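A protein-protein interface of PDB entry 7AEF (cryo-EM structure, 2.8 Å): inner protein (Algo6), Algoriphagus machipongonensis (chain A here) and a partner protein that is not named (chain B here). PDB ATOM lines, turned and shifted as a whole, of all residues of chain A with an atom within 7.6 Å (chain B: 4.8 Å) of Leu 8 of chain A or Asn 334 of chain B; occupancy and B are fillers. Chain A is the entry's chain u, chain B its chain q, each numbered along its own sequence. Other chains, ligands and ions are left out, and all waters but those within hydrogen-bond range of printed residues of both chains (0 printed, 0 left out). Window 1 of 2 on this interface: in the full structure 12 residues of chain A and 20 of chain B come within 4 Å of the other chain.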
ATOM      1  N   PRO A   2     -29.865  30.321  -0.330  1.00  0.00           N
ATOM      2  CA  PRO A   2     -30.163  29.768   0.994  1.00  0.00           C
ATOM      3  C   PRO A   2     -30.083  30.812   2.095  1.00  0.00           C
ATOM      4  O   PRO A   2     -29.325  31.765   1.973  1.00  0.00           O
ATOM      5  CB  PRO A   2     -29.083  28.699   1.176  1.00  0.00           C
ATOM      6  CG  PRO A   2     -28.015  29.048   0.205  1.00  0.00           C
ATOM      7  CD  PRO A   2     -28.710  29.657  -0.956  1.00  0.00           C
ATOM      8  N   GLU A   4     -29.064  29.986   5.056  1.00  0.00           N
ATOM      9  CA  GLU A   4     -28.200  29.289   6.000  1.00  0.00           C
ATOM     10  C   GLU A   4     -26.827  29.079   5.385  1.00  0.00           C
ATOM     11  O   GLU A   4     -26.716  28.668   4.228  1.00  0.00           O
ATOM     12  CB  GLU A   4     -28.785  27.932   6.387  1.00  0.00           C
ATOM     13  CG  GLU A   4     -30.002  27.995   7.272  1.00  0.00           C
ATOM     14  CD  GLU A   4     -30.830  26.741   7.183  1.00  0.00           C
ATOM     15  OE1 GLU A   4     -30.423  25.821   6.444  1.00  0.00           O
ATOM     16  OE2 GLU A   4     -31.886  26.669   7.846  1.00  0.00           O
ATOM     17  N   ILE A   5     -25.777  29.338   6.171  1.00  0.00           N
ATOM     18  CA  ILE A   5     -24.406  29.093   5.718  1.00  0.00           C
ATOM     19  C   ILE A   5     -24.010  27.628   5.819  1.00  0.00           C
ATOM     20  O   ILE A   5     -22.873  27.275   5.490  1.00  0.00           O
ATOM     21  CB  ILE A   5     -23.391  29.945   6.509  1.00  0.00           C
ATOM     22  CG1 ILE A   5     -23.371  29.536   7.982  1.00  0.00           C
ATOM     23  CG2 ILE A   5     -23.711  31.423   6.373  1.00  0.00           C
ATOM     24  CD1 ILE A   5     -22.089  29.810   8.673  1.00  0.00           C
ATOM     25  N   LYS A   6     -24.926  26.768   6.258  1.00  0.00           N
ATOM     26  CA  LYS A   6     -24.660  25.342   6.408  1.00  0.00           C
ATOM     27  C   LYS A   6     -24.592  24.637   5.055  1.00  0.00           C
ATOM     28  O   LYS A   6     -24.064  23.527   4.953  1.00  0.00           O
ATOM     29  CB  LYS A   6     -25.766  24.735   7.269  1.00  0.00           C
ATOM     30  CG  LYS A   6     -25.437  23.481   8.037  1.00  0.00           C
ATOM     31  CD  LYS A   6     -26.708  23.010   8.722  1.00  0.00           C
ATOM     32  CE  LYS A   6     -26.512  21.723   9.486  1.00  0.00           C
ATOM     33  NZ  LYS A   6     -27.823  21.101   9.834  1.00  0.00           N
ATOM     34  N   GLU A   7     -25.125  25.265   4.012  1.00  0.00           N
ATOM     35  CA  GLU A   7     -25.341  24.607   2.734  1.00  0.00           C
ATOM     36  C   GLU A   7     -24.443  25.125   1.620  1.00  0.00           C
ATOM     37  O   GLU A   7     -24.694  24.816   0.453  1.00  0.00           O
ATOM     38  CB  GLU A   7     -26.806  24.757   2.333  1.00  0.00           C
ATOM     39  CG  GLU A   7     -27.761  24.307   3.417  1.00  0.00           C
ATOM     40  CD  GLU A   7     -29.182  24.733   3.160  1.00  0.00           C
ATOM     41  OE1 GLU A   7     -29.399  25.544   2.238  1.00  0.00           O
ATOM     42  OE2 GLU A   7     -30.086  24.257   3.877  1.00  0.00           O
ATOM     43  N   LEU A   8     -23.409  25.893   1.940  1.00  0.00           N
ATOM     44  CA  LEU A   8     -22.492  26.374   0.919  1.00  0.00           C
ATOM     45  C   LEU A   8     -21.322  25.408   0.750  1.00  0.00           C
ATOM     46  O   LEU A   8     -20.875  24.761   1.698  1.00  0.00           O
ATOM     47  CB  LEU A   8     -21.988  27.775   1.281  1.00  0.00           C
ATOM     48  CG  LEU A   8     -23.062  28.835   1.562  1.00  0.00           C
ATOM     49  CD1 LEU A   8     -22.481  30.054   2.241  1.00  0.00           C
ATOM     50  CD2 LEU A   8     -23.792  29.239   0.294  1.00  0.00           C
ATOM     51  N   HIS A   9     -20.822  25.315  -0.480  1.00  0.00           N
ATOM     52  CA  HIS A   9     -19.725  24.427  -0.830  1.00  0.00           C
ATOM     53  C   HIS A   9     -18.508  25.262  -1.206  1.00  0.00           C
ATOM     54  O   HIS A   9     -18.641  26.402  -1.653  1.00  0.00           O
ATOM     55  CB  HIS A   9     -20.112  23.501  -1.994  1.00  0.00           C
ATOM     56  CG  HIS A   9     -19.362  22.206  -2.022  1.00  0.00           C
ATOM     57  ND1 HIS A   9     -19.558  21.211  -1.088  1.00  0.00           N
ATOM     58  CD2 HIS A   9     -18.429  21.736  -2.882  1.00  0.00           C
ATOM     59  CE1 HIS A   9     -18.769  20.187  -1.368  1.00  0.00           C
ATOM     60  NE2 HIS A   9     -18.074  20.481  -2.451  1.00  0.00           N
ATOM     61  N   ILE A  10     -17.317  24.683  -1.012  1.00  0.00           N
ATOM     62  CA  ILE A  10     -16.085  25.393  -1.330  1.00  0.00           C
ATOM     63  C   ILE A  10     -15.916  25.466  -2.845  1.00  0.00           C
ATOM     64  O   ILE A  10     -16.274  24.537  -3.580  1.00  0.00           O
ATOM     65  CB  ILE A  10     -14.887  24.732  -0.616  1.00  0.00           C
ATOM     66  CG1 ILE A  10     -13.607  25.562  -0.771  1.00  0.00           C
ATOM     67  CG2 ILE A  10     -14.682  23.279  -1.040  1.00  0.00           C
ATOM     68  CD1 ILE A  10     -12.411  25.030  -0.030  1.00  0.00           C
ATOM     69  N   LYS A  11     -15.402  26.597  -3.322  1.00  0.00           N
ATOM     70  CA  LYS A  11     -15.322  26.914  -4.742  1.00  0.00           C
ATOM     71  C   LYS A  11     -13.951  26.532  -5.289  1.00  0.00           C
ATOM     72  O   LYS A  11     -12.932  27.072  -4.850  1.00  0.00           O
ATOM     73  CB  LYS A  11     -15.605  28.403  -4.955  1.00  0.00           C
ATOM     74  CG  LYS A  11     -15.122  29.001  -6.263  1.00  0.00           C
ATOM     75  CD  LYS A  11     -15.299  30.506  -6.235  1.00  0.00           C
ATOM     76  CE  LYS A  11     -14.435  31.199  -7.267  1.00  0.00           C
ATOM     77  NZ  LYS A  11     -14.196  32.624  -6.908  1.00  0.00           N
ATOM     78  N   VAL A  39     -27.588  23.002  -6.593  1.00  0.00           N
ATOM     79  CA  VAL A  39     -27.587  22.639  -5.177  1.00  0.00           C
ATOM     80  C   VAL A  39     -28.675  23.405  -4.431  1.00  0.00           C
ATOM     81  O   VAL A  39     -29.228  22.919  -3.440  1.00  0.00           O
ATOM     82  CB  VAL A  39     -26.185  22.865  -4.569  1.00  0.00           C
ATOM     83  CG1 VAL A  39     -26.085  22.310  -3.161  1.00  0.00           C
ATOM     84  CG2 VAL A  39     -25.132  22.194  -5.412  1.00  0.00           C
ATOM     85  N   LEU A  43     -32.079  21.277  -2.446  1.00  0.00           N
ATOM     86  CA  LEU A  43     -32.298  21.392  -1.010  1.00  0.00           C
ATOM     87  C   LEU A  43     -33.612  22.084  -0.680  1.00  0.00           C
ATOM     88  O   LEU A  43     -34.102  21.962   0.444  1.00  0.00           O
ATOM     89  CB  LEU A  43     -31.128  22.136  -0.366  1.00  0.00           C
ATOM     90  CG  LEU A  43     -29.749  21.489  -0.508  1.00  0.00           C
ATOM     91  CD1 LEU A  43     -28.699  22.343   0.159  1.00  0.00           C
ATOM     92  CD2 LEU A  43     -29.730  20.077   0.047  1.00  0.00           C
ATOM     93  N   GLN B  37     -11.350  27.964   3.101  1.00  0.00           N
ATOM     94  CA  GLN B  37     -12.690  28.164   3.674  1.00  0.00           C
ATOM     95  C   GLN B  37     -12.712  28.036   5.191  1.00  0.00           C
ATOM     96  O   GLN B  37     -12.164  27.084   5.742  1.00  0.00           O
ATOM     97  CB  GLN B  37     -13.693  27.160   3.131  1.00  0.00           C
ATOM     98  CG  GLN B  37     -15.084  27.345   3.715  1.00  0.00           C
ATOM     99  CD  GLN B  37     -16.067  26.389   3.233  1.00  0.00           C
ATOM    100  OE1 GLN B  37     -15.742  25.231   2.893  1.00  0.00           O
ATOM    101  NE2 GLN B  37     -17.316  26.827   3.209  1.00  0.00           N
ATOM    102  N   VAL B  38     -13.356  28.984   5.878  1.00  0.00           N
ATOM    103  CA  VAL B  38     -13.512  28.906   7.339  1.00  0.00           C
ATOM    104  C   VAL B  38     -14.956  29.147   7.780  1.00  0.00           C
ATOM    105  O   VAL B  38     -15.586  30.114   7.350  1.00  0.00           O
ATOM    106  CB  VAL B  38     -12.599  29.909   8.086  1.00  0.00           C
ATOM    107  CG1 VAL B  38     -12.811  29.783   9.592  1.00  0.00           C
ATOM    108  CG2 VAL B  38     -11.151  29.665   7.735  1.00  0.00           C
ATOM    109  N   THR B  39     -15.488  28.275   8.643  1.00  0.00           N
ATOM    110  CA  THR B  39     -16.847  28.478   9.160  1.00  0.00           C
ATOM    111  C   THR B  39     -16.966  28.418  10.679  1.00  0.00           C
ATOM    112  O   THR B  39     -16.331  27.605  11.367  1.00  0.00           O
ATOM    113  CB  THR B  39     -17.830  27.458   8.583  1.00  0.00           C
ATOM    114  OG1 THR B  39     -17.402  26.154   8.906  1.00  0.00           O
ATOM    115  CG2 THR B  39     -17.909  27.597   7.123  1.00  0.00           C
ATOM    116  N   GLY B 332     -24.114  33.207  12.640  1.00  0.00           N
ATOM    117  CA  GLY B 332     -23.144  32.387  11.903  1.00  0.00           C
ATOM    118  C   GLY B 332     -22.351  33.157  10.853  1.00  0.00           C
ATOM    119  O   GLY B 332     -22.829  34.133  10.275  1.00  0.00           O
ATOM    120  N   VAL B 333     -21.119  32.692  10.596  1.00  0.00           N
ATOM    121  CA  VAL B 333     -20.207  33.302   9.618  1.00  0.00           C
ATOM    122  C   VAL B 333     -19.466  32.305   8.693  1.00  0.00           C
ATOM    123  O   VAL B 333     -18.897  31.308   9.143  1.00  0.00           O
ATOM    124  CB  VAL B 333     -19.168  34.187  10.359  1.00  0.00           C
ATOM    125  CG1 VAL B 333     -18.217  34.824   9.390  1.00  0.00           C
ATOM    126  CG2 VAL B 333     -19.871  35.285  11.129  1.00  0.00           C
ATOM    127  N   ASN B 334     -19.422  32.621   7.395  1.00  0.00           N
ATOM    128  CA  ASN B 334     -18.664  31.842   6.397  1.00  0.00           C
ATOM    129  C   ASN B 334     -17.672  32.685   5.583  1.00  0.00           C
ATOM    130  O   ASN B 334     -18.062  33.580   4.830  1.00  0.00           O
ATOM    131  CB  ASN B 334     -19.609  31.123   5.457  1.00  0.00           C
ATOM    132  CG  ASN B 334     -18.968  30.256   4.394  1.00  0.00           C
ATOM    133  OD1 ASN B 334     -18.134  29.385   4.643  1.00  0.00           O
ATOM    134  ND2 ASN B 334     -19.348  30.518   3.175  1.00  0.00           N
ATOM    135  N   HIS B 335     -16.376  32.406   5.757  1.00  0.00           N
ATOM    136  CA  HIS B 335     -15.289  33.119   5.071  1.00  0.00           C
ATOM    137  C   HIS B 335     -14.808  32.337   3.872  1.00  0.00           C
ATOM    138  O   HIS B 335     -14.409  31.176   3.993  1.00  0.00           O
ATOM    139  CB  HIS B 335     -14.062  33.316   5.952  1.00  0.00           C
ATOM    140  CG  HIS B 335     -14.217  34.189   7.095  1.00  0.00           C
ATOM    141  ND1 HIS B 335     -13.926  35.523   7.049  1.00  0.00           N
ATOM    142  CD2 HIS B 335     -14.625  33.931   8.337  1.00  0.00           C
ATOM    143  CE1 HIS B 335     -14.158  36.049   8.230  1.00  0.00           C
ATOM    144  NE2 HIS B 335     -14.583  35.096   9.024  1.00  0.00           N
ATOM    145  N   GLN B 336     -14.815  32.968   2.712  1.00  0.00           N
ATOM    146  CA  GLN B 336     -14.380  32.296   1.493  1.00  0.00           C
ATOM    147  C   GLN B 336     -13.282  33.077   0.787  1.00  0.00           C
ATOM    148  O   GLN B 336     -13.497  34.211   0.351  1.00  0.00           O
ATOM    149  CB  GLN B 336     -15.579  32.128   0.556  1.00  0.00           C
ATOM    150  CG  GLN B 336     -15.308  31.457  -0.789  1.00  0.00           C
ATOM    151  CD  GLN B 336     -14.998  29.971  -0.662  1.00  0.00           C
ATOM    152  OE1 GLN B 336     -15.802  29.221  -0.107  1.00  0.00           O
ATOM    153  NE2 GLN B 336     -13.872  29.530  -1.178  1.00  0.00           N
ATOM    154  N   THR B 343     -14.498  37.215   0.674  1.00  0.00           N
ATOM    155  CA  THR B 343     -15.872  37.612   0.970  1.00  0.00           C
ATOM    156  C   THR B 343     -16.390  36.887   2.196  1.00  0.00           C
ATOM    157  O   THR B 343     -15.865  35.839   2.586  1.00  0.00           O
ATOM    158  CB  THR B 343     -16.826  37.354  -0.205  1.00  0.00           C
ATOM    159  OG1 THR B 343     -16.872  35.951  -0.481  1.00  0.00           O
ATOM    160  CG2 THR B 343     -16.354  38.106  -1.423  1.00  0.00           C
ATOM    161  N   VAL B 344     -17.377  37.458   2.852  1.00  0.00           N
ATOM    162  CA  VAL B 344     -17.998  36.835   4.016  1.00  0.00           C
ATOM    163  C   VAL B 344     -19.543  36.775   3.930  1.00  0.00           C
ATOM    164  O   VAL B 344     -20.137  37.711   3.509  1.00  0.00           O
ATOM    165  CB  VAL B 344     -17.490  37.485   5.329  1.00  0.00           C
ATOM    166  CG1 VAL B 344     -17.974  38.904   5.485  1.00  0.00           C
ATOM    167  CG2 VAL B 344     -17.895  36.677   6.525  1.00  0.00           C
ATOM    168  N   ASP B 345     -20.150  35.636   4.250  1.00  0.00           N
ATOM    169  CA  ASP B 345     -21.590  35.405   4.344  1.00  0.00           C
ATOM    170  C   ASP B 345     -22.012  35.477   5.803  1.00  0.00           C
ATOM    171  O   ASP B 345     -21.592  34.652   6.621  1.00  0.00           O
ATOM    172  CB  ASP B 345     -22.011  34.018   3.880  1.00  0.00           C
ATOM    173  CG  ASP B 345     -21.914  33.683   2.418  1.00  0.00           C
ATOM    174  OD1 ASP B 345     -22.589  34.310   1.631  1.00  0.00           O
ATOM    175  OD2 ASP B 345     -21.181  32.766   2.078  1.00  0.00           O
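N of Asp 345 of chain B lies within hydrogen-bond range of O of Asn 334 of chain B (3.0 Å). The backbone carbonyl oxygen (O) of Thr 343 of chain B lies within hydrogen-bond range of the backbone NH (N) of Gln 336 of chain B. The side-chain amide nitrogen (NE2) of Gln 37 of chain B is in hydrogen-bond range of the side-chain amide oxygen (OD1) of Asn 334 of chain B, 3.0 Å away.
Ile 5 of chain A touches Val 333 of chain B (CD1 to O, 3.6 Å). Ile 5 of chain A touches Asp 345 of chain B. Leu 8 of chain A touches Asn 334 of chain B. CD1 of Leu 8 of chain A touches OD2 of Asp 345 of chain B (3.0 Å). Ile 10 of chain A touches Gln 37 of chain B. NE2 of Gln 336 of chain B touches CG1 of Ile 10 of chain A (3.998 Å). N of Lys 11 of chain A touches NE2 of Gln 336 of chain B (3.9 Å).
Of the printed residues of chain B, Ile 5 of chain A touches Val 333 and Asp 345. Of the printed residues of chain A, Gln 37 of chain B touches Ile 10 (3.6 Å). Printed residues of chain B within 4 Å of Ile 10 of chain A: Gln 37 (3.6 Å) and Gln 336 (3.998 Å). Of the printed residues of chain A, Asp 345 of chain B touches Ile 5 (3.9 Å) and Leu 8 (3.0 Å). Gly 332 of chain B touches none of the printed residues of chain A. The nearest residue of chain B that does not touch Leu 8 of chain A is Gln 37 of chain B (4.4 Å). The nearest residue of chain A that does not touch Asn 334 of chain B is Ile 5 of chain A (4.1 Å). The nearest printed residue of chain B that does not touch Ile 10 of chain A is Val 38 of chain B (7.2 Å).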
